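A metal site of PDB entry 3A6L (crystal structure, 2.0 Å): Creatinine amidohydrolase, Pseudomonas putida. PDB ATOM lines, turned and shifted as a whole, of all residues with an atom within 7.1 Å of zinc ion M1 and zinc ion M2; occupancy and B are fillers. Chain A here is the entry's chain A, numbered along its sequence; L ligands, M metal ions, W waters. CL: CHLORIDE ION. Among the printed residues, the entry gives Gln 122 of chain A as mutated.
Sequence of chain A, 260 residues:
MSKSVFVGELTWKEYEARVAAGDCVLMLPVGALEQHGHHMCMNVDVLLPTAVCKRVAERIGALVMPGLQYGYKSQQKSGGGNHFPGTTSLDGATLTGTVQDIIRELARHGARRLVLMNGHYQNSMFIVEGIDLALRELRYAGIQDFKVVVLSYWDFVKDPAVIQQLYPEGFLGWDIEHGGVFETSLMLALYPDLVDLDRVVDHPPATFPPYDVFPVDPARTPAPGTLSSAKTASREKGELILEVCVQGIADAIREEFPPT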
ATOM      1  N   GLY A  31     -28.648   7.667  15.671  1.00  0.00           N
ATOM      2  CA  GLY A  31     -27.403   6.959  15.887  1.00  0.00           C
ATOM      3  C   GLY A  31     -26.489   7.488  16.981  1.00  0.00           C
ATOM      4  O   GLY A  31     -26.924   7.774  18.100  1.00  0.00           O
ATOM      5  N   ALA A  32     -25.208   7.609  16.634  1.00  0.00           N
ATOM      6  CA  ALA A  32     -24.184   8.085  17.556  1.00  0.00           C
ATOM      7  C   ALA A  32     -22.817   8.112  16.873  1.00  0.00           C
ATOM      8  O   ALA A  32     -22.630   7.493  15.833  1.00  0.00           O
ATOM      9  CB  ALA A  32     -24.121   7.177  18.765  1.00  0.00           C
ATOM     10  N   LEU A  33     -21.887   8.860  17.462  1.00  0.00           N
ATOM     11  CA  LEU A  33     -20.514   8.958  16.972  1.00  0.00           C
ATOM     12  C   LEU A  33     -19.805   8.251  18.106  1.00  0.00           C
ATOM     13  O   LEU A  33     -19.608   8.812  19.187  1.00  0.00           O
ATOM     14  CB  LEU A  33     -20.048  10.421  16.879  1.00  0.00           C
ATOM     15  CG  LEU A  33     -18.613  10.622  16.350  1.00  0.00           C
ATOM     16  CD1 LEU A  33     -18.548  10.100  14.920  1.00  0.00           C
ATOM     17  CD2 LEU A  33     -18.206  12.095  16.390  1.00  0.00           C
ATOM     18  N   GLU A  34     -19.406   7.008  17.845  1.00  0.00           N
ATOM     19  CA  GLU A  34     -18.802   6.196  18.880  1.00  0.00           C
ATOM     20  C   GLU A  34     -17.680   5.308  18.363  1.00  0.00           C
ATOM     21  O   GLU A  34     -17.740   4.779  17.249  1.00  0.00           O
ATOM     22  CB  GLU A  34     -19.918   5.339  19.483  1.00  0.00           C
ATOM     23  CG  GLU A  34     -19.538   4.319  20.532  1.00  0.00           C
ATOM     24  CD  GLU A  34     -20.728   3.428  20.861  1.00  0.00           C
ATOM     25  OE1 GLU A  34     -21.334   2.904  19.911  1.00  0.00           O
ATOM     26  OE2 GLU A  34     -21.062   3.245  22.054  1.00  0.00           O
ATOM     27  N   GLN A  35     -16.648   5.152  19.173  1.00  0.00           N
ATOM     28  CA  GLN A  35     -15.526   4.307  18.792  1.00  0.00           C
ATOM     29  C   GLN A  35     -16.042   2.918  18.454  1.00  0.00           C
ATOM     30  O   GLN A  35     -16.924   2.395  19.146  1.00  0.00           O
ATOM     31  CB  GLN A  35     -14.519   4.199  19.956  1.00  0.00           C
ATOM     32  CG  GLN A  35     -14.991   3.399  21.192  1.00  0.00           C
ATOM     33  CD  GLN A  35     -14.956   1.884  21.009  1.00  0.00           C
ATOM     34  OE1 GLN A  35     -14.217   1.368  20.181  1.00  0.00           O
ATOM     35  NE2 GLN A  35     -15.753   1.173  21.800  1.00  0.00           N
ATOM     36  N   HIS A  36     -15.513   2.325  17.388  1.00  0.00           N
ATOM     37  CA  HIS A  36     -15.882   0.960  17.023  1.00  0.00           C
ATOM     38  C   HIS A  36     -14.644   0.129  16.718  1.00  0.00           C
ATOM     39  O   HIS A  36     -14.535  -0.467  15.653  1.00  0.00           O
ATOM     40  CB  HIS A  36     -16.818   0.947  15.805  1.00  0.00           C
ATOM     41  CG  HIS A  36     -18.258   1.181  16.154  1.00  0.00           C
ATOM     42  ND1 HIS A  36     -18.754   2.425  16.489  1.00  0.00           N
ATOM     43  CD2 HIS A  36     -19.318   0.337  16.230  1.00  0.00           C
ATOM     44  CE1 HIS A  36     -20.040   2.339  16.748  1.00  0.00           C
ATOM     45  NE2 HIS A  36     -20.409   1.083  16.595  1.00  0.00           N
ATOM     46  N   MET A  40     -12.969  -0.283  12.296  1.00  0.00           N
ATOM     47  CA  MET A  40     -14.111   0.430  11.727  1.00  0.00           C
ATOM     48  C   MET A  40     -14.176   1.906  12.120  1.00  0.00           C
ATOM     49  O   MET A  40     -13.648   2.305  13.145  1.00  0.00           O
ATOM     50  CB  MET A  40     -15.427  -0.227  12.136  1.00  0.00           C
ATOM     51  CG  MET A  40     -15.708  -1.580  11.541  1.00  0.00           C
ATOM     52  SD  MET A  40     -17.472  -1.979  11.649  1.00  0.00           S
ATOM     53  CE  MET A  40     -17.646  -2.378  13.385  1.00  0.00           C
ATOM     54  N   VAL A  44     -20.556   4.404  12.457  1.00  0.00           N
ATOM     55  CA  VAL A  44     -21.275   3.167  12.208  1.00  0.00           C
ATOM     56  C   VAL A  44     -22.741   3.221  12.650  1.00  0.00           C
ATOM     57  O   VAL A  44     -23.635   2.870  11.891  1.00  0.00           O
ATOM     58  CB  VAL A  44     -20.600   1.973  12.928  1.00  0.00           C
ATOM     59  CG1 VAL A  44     -21.482   0.744  12.875  1.00  0.00           C
ATOM     60  CG2 VAL A  44     -19.242   1.681  12.299  1.00  0.00           C
ATOM     61  N   ASP A  45     -22.978   3.663  13.895  1.00  0.00           N
ATOM     62  CA  ASP A  45     -24.326   3.743  14.452  1.00  0.00           C
ATOM     63  C   ASP A  45     -25.284   4.647  13.715  1.00  0.00           C
ATOM     64  O   ASP A  45     -26.493   4.573  13.945  1.00  0.00           O
ATOM     65  CB  ASP A  45     -24.279   4.115  15.933  1.00  0.00           C
ATOM     66  CG  ASP A  45     -23.679   3.025  16.786  1.00  0.00           C
ATOM     67  OD1 ASP A  45     -23.516   1.914  16.281  1.00  0.00           O
ATOM     68  OD2 ASP A  45     -23.377   3.273  17.968  1.00  0.00           O
ATOM     69  N   VAL A  46     -24.771   5.522  12.851  1.00  0.00           N
ATOM     70  CA  VAL A  46     -25.622   6.387  12.054  1.00  0.00           C
ATOM     71  C   VAL A  46     -25.762   5.760  10.664  1.00  0.00           C
ATOM     72  O   VAL A  46     -26.871   5.654  10.122  1.00  0.00           O
ATOM     73  CB  VAL A  46     -25.047   7.817  11.888  1.00  0.00           C
ATOM     74  CG1 VAL A  46     -25.901   8.598  10.892  1.00  0.00           C
ATOM     75  CG2 VAL A  46     -25.023   8.537  13.213  1.00  0.00           C
ATOM     76  N   LEU A  48     -25.507   2.590   9.546  1.00  0.00           N
ATOM     77  CA  LEU A  48     -26.321   1.389   9.447  1.00  0.00           C
ATOM     78  C   LEU A  48     -27.831   1.608   9.548  1.00  0.00           C
ATOM     79  O   LEU A  48     -28.573   1.144   8.688  1.00  0.00           O
ATOM     80  CB  LEU A  48     -25.868   0.369  10.491  1.00  0.00           C
ATOM     81  CG  LEU A  48     -24.395  -0.053  10.347  1.00  0.00           C
ATOM     82  CD1 LEU A  48     -24.117  -1.158  11.325  1.00  0.00           C
ATOM     83  CD2 LEU A  48     -24.099  -0.520   8.920  1.00  0.00           C
ATOM     84  N   TYR A  72     -26.852   9.066  22.977  1.00  0.00           N
ATOM     85  CA  TYR A  72     -26.536   9.050  24.384  1.00  0.00           C
ATOM     86  C   TYR A  72     -25.182   8.431  24.683  1.00  0.00           C
ATOM     87  O   TYR A  72     -24.593   7.726  23.858  1.00  0.00           O
ATOM     88  CB  TYR A  72     -27.629   8.326  25.176  1.00  0.00           C
ATOM     89  CG  TYR A  72     -27.420   8.408  26.667  1.00  0.00           C
ATOM     90  CD1 TYR A  72     -27.430   9.634  27.332  1.00  0.00           C
ATOM     91  CD2 TYR A  72     -27.139   7.258  27.402  1.00  0.00           C
ATOM     92  CE1 TYR A  72     -27.144   9.711  28.703  1.00  0.00           C
ATOM     93  CE2 TYR A  72     -26.873   7.323  28.771  1.00  0.00           C
ATOM     94  CZ  TYR A  72     -26.867   8.541  29.411  1.00  0.00           C
ATOM     95  OH  TYR A  72     -26.584   8.580  30.761  1.00  0.00           O
ATOM     96  N   SER A  74     -22.028   6.356  25.707  1.00  0.00           N
ATOM     97  CA  SER A  74     -21.659   4.972  25.495  1.00  0.00           C
ATOM     98  C   SER A  74     -21.483   4.261  26.830  1.00  0.00           C
ATOM     99  O   SER A  74     -20.755   4.731  27.707  1.00  0.00           O
ATOM    100  CB  SER A  74     -20.347   4.913  24.708  1.00  0.00           C
ATOM    101  OG  SER A  74     -19.780   3.620  24.749  1.00  0.00           O
ATOM    102  N   SER A  78     -21.934  -2.136  27.000  1.00  0.00           N
ATOM    103  CA  SER A  78     -22.737  -2.050  25.793  1.00  0.00           C
ATOM    104  C   SER A  78     -21.928  -1.543  24.618  1.00  0.00           C
ATOM    105  O   SER A  78     -22.081  -2.035  23.493  1.00  0.00           O
ATOM    106  CB  SER A  78     -23.946  -1.138  26.026  1.00  0.00           C
ATOM    107  N   GLY A  79     -21.064  -0.571  24.854  1.00  0.00           N
ATOM    108  CA  GLY A  79     -20.277  -0.026  23.770  1.00  0.00           C
ATOM    109  C   GLY A  79     -18.851   0.328  24.124  1.00  0.00           C
ATOM    110  O   GLY A  79     -18.245   1.141  23.429  1.00  0.00           O
ATOM    111  N   GLY A 119     -29.903   2.960  16.266  1.00  0.00           N
ATOM    112  CA  GLY A 119     -28.733   2.195  15.872  1.00  0.00           C
ATOM    113  C   GLY A 119     -27.655   2.197  16.953  1.00  0.00           C
ATOM    114  O   GLY A 119     -26.561   1.650  16.752  1.00  0.00           O
ATOM    115  N   HIS A 120     -27.953   2.804  18.089  1.00  0.00           N
ATOM    116  CA  HIS A 120     -27.025   2.893  19.217  1.00  0.00           C
ATOM    117  C   HIS A 120     -27.716   2.362  20.480  1.00  0.00           C
ATOM    118  O   HIS A 120     -28.695   2.944  20.954  1.00  0.00           O
ATOM    119  CB  HIS A 120     -26.584   4.357  19.396  1.00  0.00           C
ATOM    120  CG  HIS A 120     -25.759   4.622  20.616  1.00  0.00           C
ATOM    121  ND1 HIS A 120     -24.511   4.066  20.817  1.00  0.00           N
ATOM    122  CD2 HIS A 120     -25.997   5.401  21.702  1.00  0.00           C
ATOM    123  CE1 HIS A 120     -24.021   4.493  21.964  1.00  0.00           C
ATOM    124  NE2 HIS A 120     -24.899   5.310  22.517  1.00  0.00           N
ATOM    125  N   TYR A 121     -27.200   1.260  20.995  1.00  0.00           N
ATOM    126  CA  TYR A 121     -27.737   0.564  22.163  1.00  0.00           C
ATOM    127  C   TYR A 121     -28.370   1.399  23.301  1.00  0.00           C
ATOM    128  O   TYR A 121     -29.520   1.170  23.701  1.00  0.00           O
ATOM    129  CB  TYR A 121     -26.629  -0.321  22.756  1.00  0.00           C
ATOM    130  CG  TYR A 121     -27.152  -1.578  23.405  1.00  0.00           C
ATOM    131  CD1 TYR A 121     -27.719  -2.589  22.638  1.00  0.00           C
ATOM    132  CD2 TYR A 121     -27.087  -1.749  24.793  1.00  0.00           C
ATOM    133  CE1 TYR A 121     -28.227  -3.749  23.227  1.00  0.00           C
ATOM    134  CE2 TYR A 121     -27.597  -2.907  25.392  1.00  0.00           C
ATOM    135  CZ  TYR A 121     -28.160  -3.895  24.596  1.00  0.00           C
ATOM    136  OH  TYR A 121     -28.678  -5.037  25.178  1.00  0.00           O
ATOM    137  N   GLN A 122     -27.624   2.363  23.814  1.00  0.00           N
ATOM    138  CA  GLN A 122     -28.104   3.178  24.918  1.00  0.00           C
ATOM    139  C   GLN A 122     -29.135   4.281  24.617  1.00  0.00           C
ATOM    140  O   GLN A 122     -29.627   4.913  25.541  1.00  0.00           O
ATOM    141  CB  GLN A 122     -26.906   3.802  25.640  1.00  0.00           C
ATOM    142  CG  GLN A 122     -25.801   2.805  26.043  1.00  0.00           C
ATOM    143  CD  GLN A 122     -24.870   2.427  24.883  1.00  0.00           C
ATOM    144  OE1 GLN A 122     -23.735   1.989  25.096  1.00  0.00           O
ATOM    145  NE2 GLN A 122     -25.343   2.579  23.644  1.00  0.00           N
ATOM    146  N   ASN A 123     -29.464   4.507  23.346  1.00  0.00           N
ATOM    147  CA  ASN A 123     -30.423   5.568  23.010  1.00  0.00           C
ATOM    148  C   ASN A 123     -31.876   5.354  23.431  1.00  0.00           C
ATOM    149  O   ASN A 123     -32.568   6.300  23.825  1.00  0.00           O
ATOM    150  CB  ASN A 123     -30.460   5.838  21.501  1.00  0.00           C
ATOM    151  CG  ASN A 123     -29.206   6.514  20.986  1.00  0.00           C
ATOM    152  OD1 ASN A 123     -28.509   7.196  21.737  1.00  0.00           O
ATOM    153  ND2 ASN A 123     -28.929   6.342  19.699  1.00  0.00           N
ATOM    154  N   TYR A 153     -33.053  -1.841  15.011  1.00  0.00           N
ATOM    155  CA  TYR A 153     -33.020  -2.772  13.883  1.00  0.00           C
ATOM    156  C   TYR A 153     -32.444  -4.150  14.156  1.00  0.00           C
ATOM    157  O   TYR A 153     -32.824  -5.113  13.502  1.00  0.00           O
ATOM    158  CB  TYR A 153     -32.312  -2.114  12.692  1.00  0.00           C
ATOM    159  CG  TYR A 153     -30.810  -2.000  12.817  1.00  0.00           C
ATOM    160  CD1 TYR A 153     -29.990  -3.067  12.437  1.00  0.00           C
ATOM    161  CD2 TYR A 153     -30.212  -0.857  13.336  1.00  0.00           C
ATOM    162  CE1 TYR A 153     -28.602  -2.981  12.576  1.00  0.00           C
ATOM    163  CE2 TYR A 153     -28.824  -0.761  13.472  1.00  0.00           C
ATOM    164  CZ  TYR A 153     -28.033  -1.830  13.086  1.00  0.00           C
ATOM    165  OH  TYR A 153     -26.662  -1.777  13.221  1.00  0.00           O
ATOM    166  N   TRP A 154     -31.526  -4.272  15.111  1.00  0.00           N
ATOM    167  CA  TRP A 154     -30.948  -5.583  15.396  1.00  0.00           C
ATOM    168  C   TRP A 154     -31.914  -6.556  16.058  1.00  0.00           C
ATOM    169  O   TRP A 154     -31.697  -7.770  16.026  1.00  0.00           O
ATOM    170  CB  TRP A 154     -29.668  -5.442  16.244  1.00  0.00           C
ATOM    171  CG  TRP A 154     -29.831  -4.706  17.521  1.00  0.00           C
ATOM    172  CD1 TRP A 154     -30.353  -5.192  18.690  1.00  0.00           C
ATOM    173  CD2 TRP A 154     -29.498  -3.340  17.759  1.00  0.00           C
ATOM    174  NE1 TRP A 154     -30.355  -4.200  19.645  1.00  0.00           N
ATOM    175  CE2 TRP A 154     -29.845  -3.047  19.100  1.00  0.00           C
ATOM    176  CE3 TRP A 154     -28.948  -2.317  16.965  1.00  0.00           C
ATOM    177  CZ2 TRP A 154     -29.643  -1.788  19.664  1.00  0.00           C
ATOM    178  CZ3 TRP A 154     -28.757  -1.056  17.536  1.00  0.00           C
ATOM    179  CH2 TRP A 154     -29.101  -0.807  18.870  1.00  0.00           C
ATOM    180  N   GLU A 177     -22.100  -7.364  21.380  1.00  0.00           N
ATOM    181  CA  GLU A 177     -21.891  -7.282  19.933  1.00  0.00           C
ATOM    182  C   GLU A 177     -21.498  -5.869  19.517  1.00  0.00           C
ATOM    183  O   GLU A 177     -22.049  -5.323  18.567  1.00  0.00           O
ATOM    184  CB  GLU A 177     -23.160  -7.677  19.177  1.00  0.00           C
ATOM    185  CG  GLU A 177     -23.176  -9.093  18.608  1.00  0.00           C
ATOM    186  CD  GLU A 177     -22.136  -9.324  17.513  1.00  0.00           C
ATOM    187  OE1 GLU A 177     -21.773  -8.370  16.805  1.00  0.00           O
ATOM    188  OE2 GLU A 177     -21.702 -10.482  17.352  1.00  0.00           O
ATOM    189  N   HIS A 178     -20.564  -5.258  20.236  1.00  0.00           N
ATOM    190  CA  HIS A 178     -20.124  -3.915  19.863  1.00  0.00           C
ATOM    191  C   HIS A 178     -18.900  -4.037  18.979  1.00  0.00           C
ATOM    192  O   HIS A 178     -17.836  -4.472  19.433  1.00  0.00           O
ATOM    193  CB  HIS A 178     -19.775  -3.071  21.105  1.00  0.00           C
ATOM    194  CG  HIS A 178     -19.271  -1.698  20.758  1.00  0.00           C
ATOM    195  ND1 HIS A 178     -20.082  -0.719  20.224  1.00  0.00           N
ATOM    196  CD2 HIS A 178     -18.035  -1.163  20.830  1.00  0.00           C
ATOM    197  CE1 HIS A 178     -19.362   0.361  19.976  1.00  0.00           C
ATOM    198  NE2 HIS A 178     -18.107   0.115  20.328  1.00  0.00           N
ATOM    199  N   GLY A 179     -19.046  -3.650  17.710  1.00  0.00           N
ATOM    200  CA  GLY A 179     -17.938  -3.717  16.772  1.00  0.00           C
ATOM    201  C   GLY A 179     -17.545  -5.152  16.463  1.00  0.00           C
ATOM    202  O   GLY A 179     -16.405  -5.418  16.088  1.00  0.00           O
ATOM    203  N   GLU A 183     -22.196  -5.897  13.308  1.00  0.00           N
ATOM    204  CA  GLU A 183     -21.963  -4.618  12.672  1.00  0.00           C
ATOM    205  C   GLU A 183     -20.898  -4.666  11.590  1.00  0.00           C
ATOM    206  O   GLU A 183     -21.081  -4.070  10.525  1.00  0.00           O
ATOM    207  CB  GLU A 183     -21.608  -3.565  13.711  1.00  0.00           C
ATOM    208  CG  GLU A 183     -22.766  -3.213  14.591  1.00  0.00           C
ATOM    209  CD  GLU A 183     -22.469  -2.043  15.472  1.00  0.00           C
ATOM    210  OE1 GLU A 183     -21.498  -2.125  16.255  1.00  0.00           O
ATOM    211  OE2 GLU A 183     -23.206  -1.034  15.364  1.00  0.00           O
HETATM  212 CL    CL L   1     -23.583  -0.469  19.841  1.00  0.00          CL
HETATM  213 ZN    ZN M   1     -22.333   0.296  16.874  1.00  0.00          ZN
HETATM  214 ZN    ZN M   2     -23.294   2.524  19.818  1.00  0.00          ZN
HETATM  215  O   HOH W   1     -22.642   1.229  22.484  1.00  0.00           O
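Zinc ion M2 is bound by OE1 of Glu 34 (2.0 Å), OD2 of Asp 45 (2.0 Å) and ND1 of His 120 (2.2 Å).
Slightly farther from zinc ion M2 lies a chlorine (CL) of the ligand (3.0 Å).
A ring nitrogen (ND1) of His 36 sits at hydrogen-bond distance from the backbone carbonyl oxygen (O) of Glu 34 (2.7 Å).
The side-chain carboxylate of Glu 34 sits at hydrogen-bond distance from the side-chain hydroxyl of Ser 74, 3.0 Å away.
The side-chain carboxylate (OE1) of Glu 183 lies within hydrogen-bond range of the backbone NH (N) of Gly 179 (3.2 Å).
A ring nitrogen (NE2) of His 120 lies close to the side-chain amide nitrogen (NE2) of Gln 122, 3.0 Å away.
The backbone carbonyl oxygen (O) of Tyr 72 sits at hydrogen-bond distance from a ring nitrogen (NE2) of His 120 (2.8 Å).
Zinc ion M1 is bound by OD1 of Asp 45, at 2.1 Å.
A ring nitrogen (NE2) of His 36 is bound to zinc ion M1, 2.1 Å away.
Zinc ion M1 is bound by OE2 of Glu 183, 2.2 Å away.
Slightly farther from zinc ion M1 lies the side-chain carboxylate (OE1) of Glu 183 (2.6 Å).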
